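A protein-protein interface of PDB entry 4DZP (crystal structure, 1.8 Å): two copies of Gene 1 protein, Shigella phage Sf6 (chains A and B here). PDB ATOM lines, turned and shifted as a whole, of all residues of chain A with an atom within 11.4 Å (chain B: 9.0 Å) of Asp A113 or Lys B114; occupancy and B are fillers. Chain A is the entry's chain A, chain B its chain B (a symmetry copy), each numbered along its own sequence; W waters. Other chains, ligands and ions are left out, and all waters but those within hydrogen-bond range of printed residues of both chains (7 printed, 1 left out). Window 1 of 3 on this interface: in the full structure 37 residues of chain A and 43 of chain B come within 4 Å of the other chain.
Water W2 bridges O of Lys B110 (2.7 Å) and O of Arg A105 (2.8 Å). Water W5 lies within hydrogen-bond range of the backbone carbonyl oxygen (O) of Pro A108 (3.0 Å) and the side-chain hydroxyl (OG1) of Thr B116 (3.0 Å).
The backbone carbonyl oxygen of Arg A109 is in hydrogen-bond range of the side-chain amino group of Lys A114 (2.8 Å). The side-chain amide oxygen (OD1) of Asn B107 lies within hydrogen-bond range of the backbone NH (N) of Lys B110, at 3.2 Å.
Trp A101 touches Tyr B111 (CZ2 to O, 3.9 Å). O of Ala A104 touches CG of Lys B114, at 3.4 Å. O of Lys B110 touches CG of Arg A105, at 3.4 Å. Pro A108 touches Lys B114 (CB to CG, 3.8 Å). O of Lys B114 touches CA of Gly A112 (3.6 Å). Asp A113 touches Val B115. Thr B116 touches Lys A114. O of Val A115 touches CA of Asn B117 (3.4 Å).
O of Thr B116 is in hydrogen-bond range of N of Val A115 (3.1 Å). The backbone NH of Asp A113 is in hydrogen-bond range of the backbone carbonyl oxygen of Lys B114 (2.9 Å). N of Asn A117 sits at hydrogen-bond distance from O of Glu B118, at 2.9 Å. NH2 of Arg A105 is in salt-bridge range of OD1 of Asp B113 (2.9 Å). OD1 of Asn A117 sits close to OD1 of Asn B117. O of Tyr B111 is in hydrogen-bond range of NE of Arg A105 (2.9 Å). The guanidinium group (NH2) of Arg A105 lies within hydrogen-bond range of the backbone carbonyl oxygen (O) of Gly B112 (3.4 Å). The backbone carbonyl oxygen of Asp A113 sits at hydrogen-bond distance from the backbone NH of Thr B116. The side-chain hydroxyl of Thr A116 lies within hydrogen-bond range of the side-chain carboxylate of Glu B118, at 2.6 Å. The backbone NH of Glu B118 sits at hydrogen-bond distance from the backbone carbonyl oxygen of Val A115, 2.8 Å away.
Val A115 touches Thr B116, but with the chains exchanged Thr A116 does not touch Val B115 (7.5 Å). Val A115 touches Asn B117, but with the chains exchanged Asn A117 does not touch Val B115 (6.5 Å). Asn B117 touches its own counterpart, Asn A117.
Of the 23 printed residues of chain A, 10 touch a printed residue of chain B. Hydrophobic or aromatic side chains of chain A that line the printed part of chain B: Trp A101, Pro A108 and Val A115. Of the 13 printed residues of chain B, 9 touch a printed residue of chain A. Hydrophobic or aromatic side chains of chain B that line the printed part of chain A: Tyr B111 and Val B115. Along chain B the printed residues that touch a printed residue of chain A span positions 110 to 118.
Of chain A, only Ala A104 (3.4 Å), Pro A108 (3.8 Å), Gly A112 (3.6 Å) and Asp A113 (2.9 Å) come within 4 Å of Lys B114. Gly B112 touches one residue of chain A. Asp B113 touches just one residue of chain A: Arg A105 (2.9 Å). Of the printed residues of chain A, Val B115 touches Asp A113 (3.5 Å). Thr B116 touches just these residues of chain A: Asp A113, Lys A114 and Val A115. Of the printed residues of chain A, Lys B110 touches Arg A105. Printed residues of chain A within 4 Å of Tyr B111: Trp A101 and Arg A105. Printed residues of chain A within 4 Å of Asn B117: Val A115 and Asn A117. Printed residues of chain B within 4 Å of Thr A116: Glu B118. The nearest residue of chain A that does not touch Lys B114 is Arg A105 (4.5 Å).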
ATOM      1  N   THR A  64      27.606  -3.770 -16.655  1.00  0.00           N
ATOM      2  CA  THR A  64      27.307  -4.960 -15.863  1.00  0.00           C
ATOM      3  C   THR A  64      27.983  -6.182 -16.482  1.00  0.00           C
ATOM      4  O   THR A  64      28.454  -7.072 -15.778  1.00  0.00           O
ATOM      5  CB  THR A  64      25.786  -5.194 -15.755  1.00  0.00           C
ATOM      6  OG1 THR A  64      25.190  -4.128 -14.999  1.00  0.00           O
ATOM      7  CG2 THR A  64      25.489  -6.531 -15.074  1.00  0.00           C
ATOM      8  N   GLU A  65      28.029  -6.233 -17.806  1.00  0.00           N
ATOM      9  CA  GLU A  65      28.728  -7.332 -18.466  1.00  0.00           C
ATOM     10  C   GLU A  65      30.246  -7.234 -18.265  1.00  0.00           C
ATOM     11  O   GLU A  65      30.929  -8.248 -18.108  1.00  0.00           O
ATOM     12  CB  GLU A  65      28.340  -7.414 -19.943  1.00  0.00           C
ATOM     13  CG  GLU A  65      26.900  -7.889 -20.157  1.00  0.00           C
ATOM     14  CD  GLU A  65      26.556  -8.108 -21.627  1.00  0.00           C
ATOM     15  OE1 GLU A  65      27.404  -7.802 -22.492  1.00  0.00           O
ATOM     16  OE2 GLU A  65      25.439  -8.595 -21.917  1.00  0.00           O
ATOM     17  N   PHE A  72      34.599 -12.820 -12.814  1.00  0.00           N
ATOM     18  CA  PHE A  72      35.011 -14.151 -13.279  1.00  0.00           C
ATOM     19  C   PHE A  72      36.464 -14.440 -12.912  1.00  0.00           C
ATOM     20  O   PHE A  72      36.820 -15.556 -12.537  1.00  0.00           O
ATOM     21  CB  PHE A  72      34.815 -14.277 -14.789  1.00  0.00           C
ATOM     22  CG  PHE A  72      35.180 -15.634 -15.346  1.00  0.00           C
ATOM     23  CD1 PHE A  72      34.301 -16.696 -15.247  1.00  0.00           C
ATOM     24  CD2 PHE A  72      36.385 -15.830 -16.002  1.00  0.00           C
ATOM     25  CE1 PHE A  72      34.622 -17.946 -15.774  1.00  0.00           C
ATOM     26  CE2 PHE A  72      36.712 -17.077 -16.529  1.00  0.00           C
ATOM     27  CZ  PHE A  72      35.815 -18.131 -16.410  1.00  0.00           C
ATOM     28  N   ASP A  97      30.523 -19.056  -4.464  1.00  0.00           N
ATOM     29  CA  ASP A  97      29.200 -19.525  -4.872  1.00  0.00           C
ATOM     30  C   ASP A  97      28.262 -18.371  -5.184  1.00  0.00           C
ATOM     31  O   ASP A  97      27.466 -18.433  -6.112  1.00  0.00           O
ATOM     32  CB  ASP A  97      28.599 -20.437  -3.794  1.00  0.00           C
ATOM     33  CG  ASP A  97      29.279 -21.802  -3.737  1.00  0.00           C
ATOM     34  OD1 ASP A  97      30.112 -22.104  -4.630  1.00  0.00           O
ATOM     35  OD2 ASP A  97      28.975 -22.578  -2.805  1.00  0.00           O
ATOM     36  N   ARG A  99      29.142 -15.359  -6.206  1.00  0.00           N
ATOM     37  CA  ARG A  99      29.590 -14.778  -7.464  1.00  0.00           C
ATOM     38  C   ARG A  99      29.203 -15.643  -8.669  1.00  0.00           C
ATOM     39  O   ARG A  99      28.776 -15.113  -9.694  1.00  0.00           O
ATOM     40  CB  ARG A  99      31.099 -14.542  -7.420  1.00  0.00           C
ATOM     41  CG  ARG A  99      31.471 -13.301  -6.599  1.00  0.00           C
ATOM     42  CD  ARG A  99      32.931 -13.320  -6.170  1.00  0.00           C
ATOM     43  NE  ARG A  99      33.299 -12.042  -5.548  1.00  0.00           N
ATOM     44  CZ  ARG A  99      32.963 -11.681  -4.315  1.00  0.00           C
ATOM     45  NH1 ARG A  99      32.242 -12.498  -3.550  1.00  0.00           N
ATOM     46  NH2 ARG A  99      33.352 -10.493  -3.847  1.00  0.00           N
ATOM     47  N   LYS A 100      29.343 -16.958  -8.550  1.00  0.00           N
ATOM     48  CA  LYS A 100      28.992 -17.841  -9.671  1.00  0.00           C
ATOM     49  C   LYS A 100      27.528 -17.665 -10.033  1.00  0.00           C
ATOM     50  O   LYS A 100      27.169 -17.574 -11.213  1.00  0.00           O
ATOM     51  CB  LYS A 100      29.279 -19.313  -9.341  1.00  0.00           C
ATOM     52  CG  LYS A 100      30.763 -19.651  -9.272  1.00  0.00           C
ATOM     53  CD  LYS A 100      30.983 -21.138  -9.045  1.00  0.00           C
ATOM     54  CE  LYS A 100      30.198 -21.679  -7.898  1.00  0.00           C
ATOM     55  NZ  LYS A 100      30.433 -23.153  -7.730  1.00  0.00           N
ATOM     56  N   TRP A 101      26.681 -17.615  -9.010  1.00  0.00           N
ATOM     57  CA  TRP A 101      25.252 -17.494  -9.216  1.00  0.00           C
ATOM     58  C   TRP A 101      24.964 -16.142  -9.867  1.00  0.00           C
ATOM     59  O   TRP A 101      24.210 -16.040 -10.841  1.00  0.00           O
ATOM     60  CB  TRP A 101      24.531 -17.625  -7.862  1.00  0.00           C
ATOM     61  CG  TRP A 101      23.020 -17.616  -7.940  1.00  0.00           C
ATOM     62  CD1 TRP A 101      22.189 -18.705  -8.067  1.00  0.00           C
ATOM     63  CD2 TRP A 101      22.174 -16.473  -7.854  1.00  0.00           C
ATOM     64  NE1 TRP A 101      20.872 -18.291  -8.082  1.00  0.00           N
ATOM     65  CE2 TRP A 101      20.835 -16.933  -7.953  1.00  0.00           C
ATOM     66  CE3 TRP A 101      22.413 -15.104  -7.720  1.00  0.00           C
ATOM     67  CZ2 TRP A 101      19.748 -16.063  -7.918  1.00  0.00           C
ATOM     68  CZ3 TRP A 101      21.319 -14.241  -7.676  1.00  0.00           C
ATOM     69  CH2 TRP A 101      20.009 -14.732  -7.776  1.00  0.00           C
ATOM     70  N   ALA A 102      25.608 -15.103  -9.355  1.00  0.00           N
ATOM     71  CA  ALA A 102      25.384 -13.756  -9.862  1.00  0.00           C
ATOM     72  C   ALA A 102      25.829 -13.595 -11.308  1.00  0.00           C
ATOM     73  O   ALA A 102      25.179 -12.888 -12.082  1.00  0.00           O
ATOM     74  CB  ALA A 102      26.084 -12.736  -8.979  1.00  0.00           C
ATOM     75  N   LEU A 103      26.951 -14.220 -11.663  1.00  0.00           N
ATOM     76  CA  LEU A 103      27.507 -14.064 -13.007  1.00  0.00           C
ATOM     77  C   LEU A 103      26.514 -14.527 -14.073  1.00  0.00           C
ATOM     78  O   LEU A 103      26.389 -13.912 -15.132  1.00  0.00           O
ATOM     79  CB  LEU A 103      28.805 -14.859 -13.125  1.00  0.00           C
ATOM     80  CG  LEU A 103      30.128 -14.076 -13.035  1.00  0.00           C
ATOM     81  CD1 LEU A 103      30.039 -12.945 -12.046  1.00  0.00           C
ATOM     82  CD2 LEU A 103      31.279 -15.042 -12.693  1.00  0.00           C
ATOM     83  N   ALA A 104      25.812 -15.621 -13.793  1.00  0.00           N
ATOM     84  CA  ALA A 104      24.850 -16.140 -14.764  1.00  0.00           C
ATOM     85  C   ALA A 104      23.739 -15.123 -15.010  1.00  0.00           C
ATOM     86  O   ALA A 104      23.173 -15.056 -16.102  1.00  0.00           O
ATOM     87  CB  ALA A 104      24.267 -17.489 -14.312  1.00  0.00           C
ATOM     88  N   ARG A 105      23.419 -14.325 -13.995  1.00  0.00           N
ATOM     89  CA  ARG A 105      22.391 -13.303 -14.167  1.00  0.00           C
ATOM     90  C   ARG A 105      22.920 -12.036 -14.836  1.00  0.00           C
ATOM     91  O   ARG A 105      22.169 -11.318 -15.506  1.00  0.00           O
ATOM     92  CB  ARG A 105      21.713 -12.964 -12.839  1.00  0.00           C
ATOM     93  CG  ARG A 105      20.609 -13.954 -12.460  1.00  0.00           C
ATOM     94  CD  ARG A 105      21.111 -14.963 -11.479  1.00  0.00           C
ATOM     95  NE  ARG A 105      20.108 -15.999 -11.206  1.00  0.00           N
ATOM     96  CZ  ARG A 105      20.389 -17.291 -11.098  1.00  0.00           C
ATOM     97  NH1 ARG A 105      21.639 -17.718 -11.237  1.00  0.00           N
ATOM     98  NH2 ARG A 105      19.420 -18.157 -10.845  1.00  0.00           N
ATOM     99  N   MET A 106      24.203 -11.750 -14.648  1.00  0.00           N
ATOM    100  CA  MET A 106      24.774 -10.551 -15.255  1.00  0.00           C
ATOM    101  C   MET A 106      25.027 -10.727 -16.750  1.00  0.00           C
ATOM    102  O   MET A 106      24.862  -9.783 -17.534  1.00  0.00           O
ATOM    103  CB  MET A 106      26.057 -10.153 -14.534  1.00  0.00           C
ATOM    104  CG  MET A 106      25.831  -9.849 -13.064  1.00  0.00           C
ATOM    105  SD  MET A 106      27.407  -9.591 -12.237  1.00  0.00           S
ATOM    106  CE  MET A 106      26.895  -9.233 -10.568  1.00  0.00           C
ATOM    107  N   ASN A 107      25.423 -11.934 -17.146  1.00  0.00           N
ATOM    108  CA  ASN A 107      25.582 -12.245 -18.563  1.00  0.00           C
ATOM    109  C   ASN A 107      25.134 -13.677 -18.842  1.00  0.00           C
ATOM    110  O   ASN A 107      25.945 -14.599 -18.843  1.00  0.00           O
ATOM    111  CB  ASN A 107      27.028 -12.015 -19.019  1.00  0.00           C
ATOM    112  CG  ASN A 107      27.178 -12.089 -20.529  1.00  0.00           C
ATOM    113  OD1 ASN A 107      26.302 -12.608 -21.227  1.00  0.00           O
ATOM    114  ND2 ASN A 107      28.296 -11.581 -21.041  1.00  0.00           N
ATOM    115  N   PRO A 108      23.828 -13.872 -19.046  1.00  0.00           N
ATOM    116  CA  PRO A 108      23.321 -15.249 -19.119  1.00  0.00           C
ATOM    117  C   PRO A 108      23.866 -16.049 -20.294  1.00  0.00           C
ATOM    118  O   PRO A 108      24.090 -17.261 -20.177  1.00  0.00           O
ATOM    119  CB  PRO A 108      21.812 -15.058 -19.276  1.00  0.00           C
ATOM    120  CG  PRO A 108      21.528 -13.714 -18.708  1.00  0.00           C
ATOM    121  CD  PRO A 108      22.740 -12.876 -18.988  1.00  0.00           C
ATOM    122  N   ARG A 109      24.051 -15.398 -21.431  1.00  0.00           N
ATOM    123  CA  ARG A 109      24.543 -16.113 -22.603  1.00  0.00           C
ATOM    124  C   ARG A 109      25.962 -16.634 -22.369  1.00  0.00           C
ATOM    125  O   ARG A 109      26.319 -17.720 -22.833  1.00  0.00           O
ATOM    126  CB  ARG A 109      24.470 -15.221 -23.849  1.00  0.00           C
ATOM    127  CG  ARG A 109      24.606 -15.986 -25.159  1.00  0.00           C
ATOM    128  CD  ARG A 109      23.929 -15.272 -26.338  1.00  0.00           C
ATOM    129  NE  ARG A 109      24.427 -13.912 -26.548  1.00  0.00           N
ATOM    130  CZ  ARG A 109      23.662 -12.823 -26.598  1.00  0.00           C
ATOM    131  NH1 ARG A 109      22.345 -12.916 -26.450  1.00  0.00           N
ATOM    132  NH2 ARG A 109      24.219 -11.632 -26.791  1.00  0.00           N
ATOM    133  N   LYS A 110      26.758 -15.873 -21.621  1.00  0.00           N
ATOM    134  CA  LYS A 110      28.150 -16.227 -21.379  1.00  0.00           C
ATOM    135  C   LYS A 110      28.361 -17.112 -20.145  1.00  0.00           C
ATOM    136  O   LYS A 110      29.102 -18.105 -20.188  1.00  0.00           O
ATOM    137  CB  LYS A 110      28.989 -14.962 -21.256  1.00  0.00           C
ATOM    138  CG  LYS A 110      30.426 -15.210 -20.906  1.00  0.00           C
ATOM    139  CD  LYS A 110      31.282 -14.005 -21.308  1.00  0.00           C
ATOM    140  CE  LYS A 110      32.752 -14.378 -21.321  1.00  0.00           C
ATOM    141  NZ  LYS A 110      33.598 -13.164 -21.538  1.00  0.00           N
ATOM    142  N   TYR A 111      27.701 -16.752 -19.052  1.00  0.00           N
ATOM    143  CA  TYR A 111      27.972 -17.387 -17.766  1.00  0.00           C
ATOM    144  C   TYR A 111      26.861 -18.316 -17.289  1.00  0.00           C
ATOM    145  O   TYR A 111      26.959 -18.868 -16.202  1.00  0.00           O
ATOM    146  CB  TYR A 111      28.284 -16.314 -16.711  1.00  0.00           C
ATOM    147  CG  TYR A 111      29.580 -15.587 -17.016  1.00  0.00           C
ATOM    148  CD1 TYR A 111      30.774 -16.293 -17.143  1.00  0.00           C
ATOM    149  CD2 TYR A 111      29.609 -14.208 -17.185  1.00  0.00           C
ATOM    150  CE1 TYR A 111      31.973 -15.638 -17.438  1.00  0.00           C
ATOM    151  CE2 TYR A 111      30.801 -13.545 -17.469  1.00  0.00           C
ATOM    152  CZ  TYR A 111      31.973 -14.271 -17.588  1.00  0.00           C
ATOM    153  OH  TYR A 111      33.162 -13.625 -17.877  1.00  0.00           O
ATOM    154  N   GLY A 112      25.815 -18.486 -18.088  1.00  0.00           N
ATOM    155  CA  GLY A 112      24.781 -19.455 -17.744  1.00  0.00           C
ATOM    156  C   GLY A 112      25.307 -20.892 -17.806  1.00  0.00           C
ATOM    157  O   GLY A 112      26.419 -21.138 -18.276  1.00  0.00           O
ATOM    158  N   ASP A 113      24.496 -21.845 -17.342  1.00  0.00           N
ATOM    159  CA  ASP A 113      24.876 -23.250 -17.368  1.00  0.00           C
ATOM    160  C   ASP A 113      24.974 -23.718 -18.806  1.00  0.00           C
ATOM    161  O   ASP A 113      24.300 -23.186 -19.685  1.00  0.00           O
ATOM    162  CB  ASP A 113      23.828 -24.114 -16.641  1.00  0.00           C
ATOM    163  CG  ASP A 113      23.952 -24.065 -15.126  1.00  0.00           C
ATOM    164  OD1 ASP A 113      24.910 -23.456 -14.581  1.00  0.00           O
ATOM    165  OD2 ASP A 113      23.063 -24.650 -14.471  1.00  0.00           O
ATOM    166  N   LYS A 114      25.777 -24.754 -19.026  1.00  0.00           N
ATOM    167  CA  LYS A 114      26.027 -25.280 -20.357  1.00  0.00           C
ATOM    168  C   LYS A 114      25.747 -26.764 -20.337  1.00  0.00           C
ATOM    169  O   LYS A 114      26.387 -27.483 -19.587  1.00  0.00           O
ATOM    170  CB  LYS A 114      27.496 -25.071 -20.736  1.00  0.00           C
ATOM    171  CG  LYS A 114      28.001 -23.650 -20.480  1.00  0.00           C
ATOM    172  CD  LYS A 114      27.343 -22.688 -21.447  1.00  0.00           C
ATOM    173  CE  LYS A 114      27.850 -21.265 -21.168  1.00  0.00           C
ATOM    174  NZ  LYS A 114      27.034 -20.300 -21.938  1.00  0.00           N
ATOM    175  N   VAL A 115      24.792 -27.216 -21.147  1.00  0.00           N
ATOM    176  CA  VAL A 115      24.484 -28.639 -21.229  1.00  0.00           C
ATOM    177  C   VAL A 115      24.391 -29.048 -22.699  1.00  0.00           C
ATOM    178  O   VAL A 115      23.913 -28.272 -23.528  1.00  0.00           O
ATOM    179  CB  VAL A 115      23.136 -28.993 -20.523  1.00  0.00           C
ATOM    180  CG1 VAL A 115      22.939 -30.508 -20.531  1.00  0.00           C
ATOM    181  CG2 VAL A 115      23.110 -28.478 -19.088  1.00  0.00           C
ATOM    182  N   THR A 116      24.857 -30.253 -23.024  1.00  0.00           N
ATOM    183  CA  THR A 116      24.603 -30.822 -24.341  1.00  0.00           C
ATOM    184  C   THR A 116      23.716 -32.018 -24.085  1.00  0.00           C
ATOM    185  O   THR A 116      24.113 -32.925 -23.363  1.00  0.00           O
ATOM    186  CB  THR A 116      25.906 -31.268 -25.042  1.00  0.00           C
ATOM    187  OG1 THR A 116      26.749 -30.117 -25.242  1.00  0.00           O
ATOM    188  CG2 THR A 116      25.604 -31.923 -26.390  1.00  0.00           C
ATOM    189  N   ASN A 117      22.508 -31.997 -24.642  1.00  0.00           N
ATOM    190  CA  ASN A 117      21.562 -33.095 -24.469  1.00  0.00           C
ATOM    191  C   ASN A 117      21.493 -33.903 -25.746  1.00  0.00           C
ATOM    192  O   ASN A 117      21.078 -33.376 -26.775  1.00  0.00           O
ATOM    193  CB  ASN A 117      20.155 -32.545 -24.201  1.00  0.00           C
ATOM    194  CG  ASN A 117      20.087 -31.702 -22.956  1.00  0.00           C
ATOM    195  OD1 ASN A 117      20.311 -30.489 -23.007  1.00  0.00           O
ATOM    196  ND2 ASN A 117      19.753 -32.333 -21.824  1.00  0.00           N
ATOM    197  N   ALA B 104      14.593 -15.138  -7.728  1.00  0.00           N
ATOM    198  CA  ALA B 104      14.048 -15.768  -8.928  1.00  0.00           C
ATOM    199  C   ALA B 104      12.518 -15.666  -8.965  1.00  0.00           C
ATOM    200  O   ALA B 104      11.923 -15.591 -10.034  1.00  0.00           O
ATOM    201  CB  ALA B 104      14.495 -17.231  -9.040  1.00  0.00           C
ATOM    202  N   ASN B 107      11.475 -11.692  -9.646  1.00  0.00           N
ATOM    203  CA  ASN B 107      11.649 -11.308 -11.045  1.00  0.00           C
ATOM    204  C   ASN B 107      12.235 -12.481 -11.834  1.00  0.00           C
ATOM    205  O   ASN B 107      13.445 -12.542 -12.031  1.00  0.00           O
ATOM    206  CB  ASN B 107      12.587 -10.100 -11.162  1.00  0.00           C
ATOM    207  CG  ASN B 107      12.591  -9.489 -12.552  1.00  0.00           C
ATOM    208  OD1 ASN B 107      12.280 -10.156 -13.544  1.00  0.00           O
ATOM    209  ND2 ASN B 107      12.970  -8.214 -12.635  1.00  0.00           N
ATOM    210  N   PRO B 108      11.374 -13.415 -12.261  1.00  0.00           N
ATOM    211  CA  PRO B 108      11.810 -14.670 -12.886  1.00  0.00           C
ATOM    212  C   PRO B 108      12.616 -14.431 -14.147  1.00  0.00           C
ATOM    213  O   PRO B 108      13.582 -15.156 -14.413  1.00  0.00           O
ATOM    214  CB  PRO B 108      10.493 -15.355 -13.247  1.00  0.00           C
ATOM    215  CG  PRO B 108       9.494 -14.786 -12.325  1.00  0.00           C
ATOM    216  CD  PRO B 108       9.912 -13.369 -12.072  1.00  0.00           C
ATOM    217  N   ARG B 109      12.233 -13.415 -14.915  1.00  0.00           N
ATOM    218  CA  ARG B 109      12.897 -13.152 -16.190  1.00  0.00           C
ATOM    219  C   ARG B 109      14.345 -12.739 -15.983  1.00  0.00           C
ATOM    220  O   ARG B 109      15.241 -13.153 -16.719  1.00  0.00           O
ATOM    221  CB  ARG B 109      12.145 -12.063 -16.952  1.00  0.00           C
ATOM    222  CG  ARG B 109      12.015 -12.314 -18.435  1.00  0.00           C
ATOM    223  CD  ARG B 109      10.813 -11.563 -18.990  1.00  0.00           C
ATOM    224  NE  ARG B 109      10.948 -10.117 -18.822  1.00  0.00           N
ATOM    225  CZ  ARG B 109       9.959  -9.248 -19.010  1.00  0.00           C
ATOM    226  NH1 ARG B 109       8.757  -9.678 -19.367  1.00  0.00           N
ATOM    227  NH2 ARG B 109      10.170  -7.950 -18.837  1.00  0.00           N
ATOM    228  N   LYS B 110      14.572 -11.903 -14.979  1.00  0.00           N
ATOM    229  CA  LYS B 110      15.906 -11.419 -14.684  1.00  0.00           C
ATOM    230  C   LYS B 110      16.744 -12.391 -13.839  1.00  0.00           C
ATOM    231  O   LYS B 110      17.927 -12.599 -14.104  1.00  0.00           O
ATOM    232  CB  LYS B 110      15.804 -10.075 -13.978  1.00  0.00           C
ATOM    233  CG  LYS B 110      17.113  -9.357 -13.854  1.00  0.00           C
ATOM    234  CD  LYS B 110      16.881  -7.881 -13.526  1.00  0.00           C
ATOM    235  CE  LYS B 110      18.209  -7.193 -13.294  1.00  0.00           C
ATOM    236  NZ  LYS B 110      18.021  -5.811 -12.765  1.00  0.00           N
ATOM    237  N   TYR B 111      16.132 -12.983 -12.821  1.00  0.00           N
ATOM    238  CA  TYR B 111      16.899 -13.699 -11.815  1.00  0.00           C
ATOM    239  C   TYR B 111      16.667 -15.204 -11.785  1.00  0.00           C
ATOM    240  O   TYR B 111      17.229 -15.872 -10.933  1.00  0.00           O
ATOM    241  CB  TYR B 111      16.635 -13.113 -10.421  1.00  0.00           C
ATOM    242  CG  TYR B 111      17.090 -11.680 -10.290  1.00  0.00           C
ATOM    243  CD1 TYR B 111      18.431 -11.352 -10.420  1.00  0.00           C
ATOM    244  CD2 TYR B 111      16.182 -10.664 -10.016  1.00  0.00           C
ATOM    245  CE1 TYR B 111      18.855 -10.039 -10.316  1.00  0.00           C
ATOM    246  CE2 TYR B 111      16.599  -9.355  -9.889  1.00  0.00           C
ATOM    247  CZ  TYR B 111      17.934  -9.051 -10.037  1.00  0.00           C
ATOM    248  OH  TYR B 111      18.356  -7.743  -9.924  1.00  0.00           O
ATOM    249  N   GLY B 112      15.853 -15.730 -12.698  1.00  0.00           N
ATOM    250  CA  GLY B 112      15.735 -17.177 -12.822  1.00  0.00           C
ATOM    251  C   GLY B 112      17.035 -17.800 -13.295  1.00  0.00           C
ATOM    252  O   GLY B 112      17.955 -17.096 -13.708  1.00  0.00           O
ATOM    253  N   ASP B 113      17.092 -19.130 -13.252  1.00  0.00           N
ATOM    254  CA  ASP B 113      18.253 -19.865 -13.721  1.00  0.00           C
ATOM    255  C   ASP B 113      18.413 -19.656 -15.216  1.00  0.00           C
ATOM    256  O   ASP B 113      17.432 -19.426 -15.923  1.00  0.00           O
ATOM    257  CB  ASP B 113      18.066 -21.371 -13.462  1.00  0.00           C
ATOM    258  CG  ASP B 113      18.290 -21.766 -12.002  1.00  0.00           C
ATOM    259  OD1 ASP B 113      18.674 -20.909 -11.164  1.00  0.00           O
ATOM    260  OD2 ASP B 113      18.078 -22.965 -11.698  1.00  0.00           O
ATOM    261  N   LYS B 114      19.653 -19.786 -15.688  1.00  0.00           N
ATOM    262  CA  LYS B 114      20.004 -19.570 -17.085  1.00  0.00           C
ATOM    263  C   LYS B 114      20.738 -20.806 -17.576  1.00  0.00           C
ATOM    264  O   LYS B 114      21.736 -21.193 -16.989  1.00  0.00           O
ATOM    265  CB  LYS B 114      20.936 -18.363 -17.210  1.00  0.00           C
ATOM    266  CG  LYS B 114      20.460 -17.136 -16.450  1.00  0.00           C
ATOM    267  CD  LYS B 114      19.187 -16.628 -17.060  1.00  0.00           C
ATOM    268  CE  LYS B 114      18.833 -15.280 -16.413  1.00  0.00           C
ATOM    269  NZ  LYS B 114      17.437 -14.932 -16.646  1.00  0.00           N
ATOM    270  N   VAL B 115      20.216 -21.442 -18.624  1.00  0.00           N
ATOM    271  CA  VAL B 115      20.853 -22.635 -19.170  1.00  0.00           C
ATOM    272  C   VAL B 115      20.868 -22.515 -20.678  1.00  0.00           C
ATOM    273  O   VAL B 115      19.900 -22.032 -21.264  1.00  0.00           O
ATOM    274  CB  VAL B 115      20.075 -23.923 -18.816  1.00  0.00           C
ATOM    275  CG1 VAL B 115      20.826 -25.140 -19.361  1.00  0.00           C
ATOM    276  CG2 VAL B 115      19.859 -24.051 -17.300  1.00  0.00           C
ATOM    277  N   THR B 116      21.970 -22.929 -21.309  1.00  0.00           N
ATOM    278  CA  THR B 116      21.983 -23.068 -22.766  1.00  0.00           C
ATOM    279  C   THR B 116      22.072 -24.567 -23.063  1.00  0.00           C
ATOM    280  O   THR B 116      23.023 -25.226 -22.639  1.00  0.00           O
ATOM    281  CB  THR B 116      23.194 -22.349 -23.399  1.00  0.00           C
ATOM    282  OG1 THR B 116      23.111 -20.938 -23.122  1.00  0.00           O
ATOM    283  CG2 THR B 116      23.207 -22.565 -24.907  1.00  0.00           C
ATOM    284  N   ASN B 117      21.067 -25.117 -23.746  1.00  0.00           N
ATOM    285  CA  ASN B 117      21.053 -26.554 -24.053  1.00  0.00           C
ATOM    286  C   ASN B 117      21.382 -26.740 -25.519  1.00  0.00           C
ATOM    287  O   ASN B 117      20.631 -26.274 -26.385  1.00  0.00           O
ATOM    288  CB  ASN B 117      19.663 -27.163 -23.798  1.00  0.00           C
ATOM    289  CG  ASN B 117      19.223 -27.070 -22.342  1.00  0.00           C
ATOM    290  OD1 ASN B 117      19.448 -27.991 -21.536  1.00  0.00           O
ATOM    291  ND2 ASN B 117      18.571 -25.969 -22.002  1.00  0.00           N
ATOM    292  N   GLU B 118      22.505 -27.397 -25.796  1.00  0.00           N
ATOM    293  CA  GLU B 118      22.862 -27.768 -27.157  1.00  0.00           C
ATOM    294  C   GLU B 118      22.180 -29.097 -27.416  1.00  0.00           C
ATOM    295  O   GLU B 118      22.514 -30.095 -26.790  1.00  0.00           O
ATOM    296  CB  GLU B 118      24.388 -27.904 -27.287  1.00  0.00           C
ATOM    297  CG  GLU B 118      24.851 -28.444 -28.647  1.00  0.00           C
ATOM    298  CD  GLU B 118      26.341 -28.784 -28.695  1.00  0.00           C
ATOM    299  OE1 GLU B 118      26.922 -29.138 -27.638  1.00  0.00           O
ATOM    300  OE2 GLU B 118      26.930 -28.718 -29.804  1.00  0.00           O
HETATM  301  O   HOH W   1      25.729 -25.339 -23.964  1.00  0.00           O
HETATM  302  O   HOH W   2      19.510 -11.769 -16.095  1.00  0.00           O
HETATM  303  O   HOH W   3      16.536 -19.565  -9.925  1.00  0.00           O
HETATM  304  O   HOH W   4      24.943 -19.252 -24.750  1.00  0.00           O
HETATM  305  O   HOH W   5      21.931 -18.999 -21.215  1.00  0.00           O
HETATM  306  O   HOH W   6      19.649 -21.201  -8.765  1.00  0.00           O
HETATM  307  O   HOH W   7      29.271 -30.442 -27.223  1.00  0.00           O
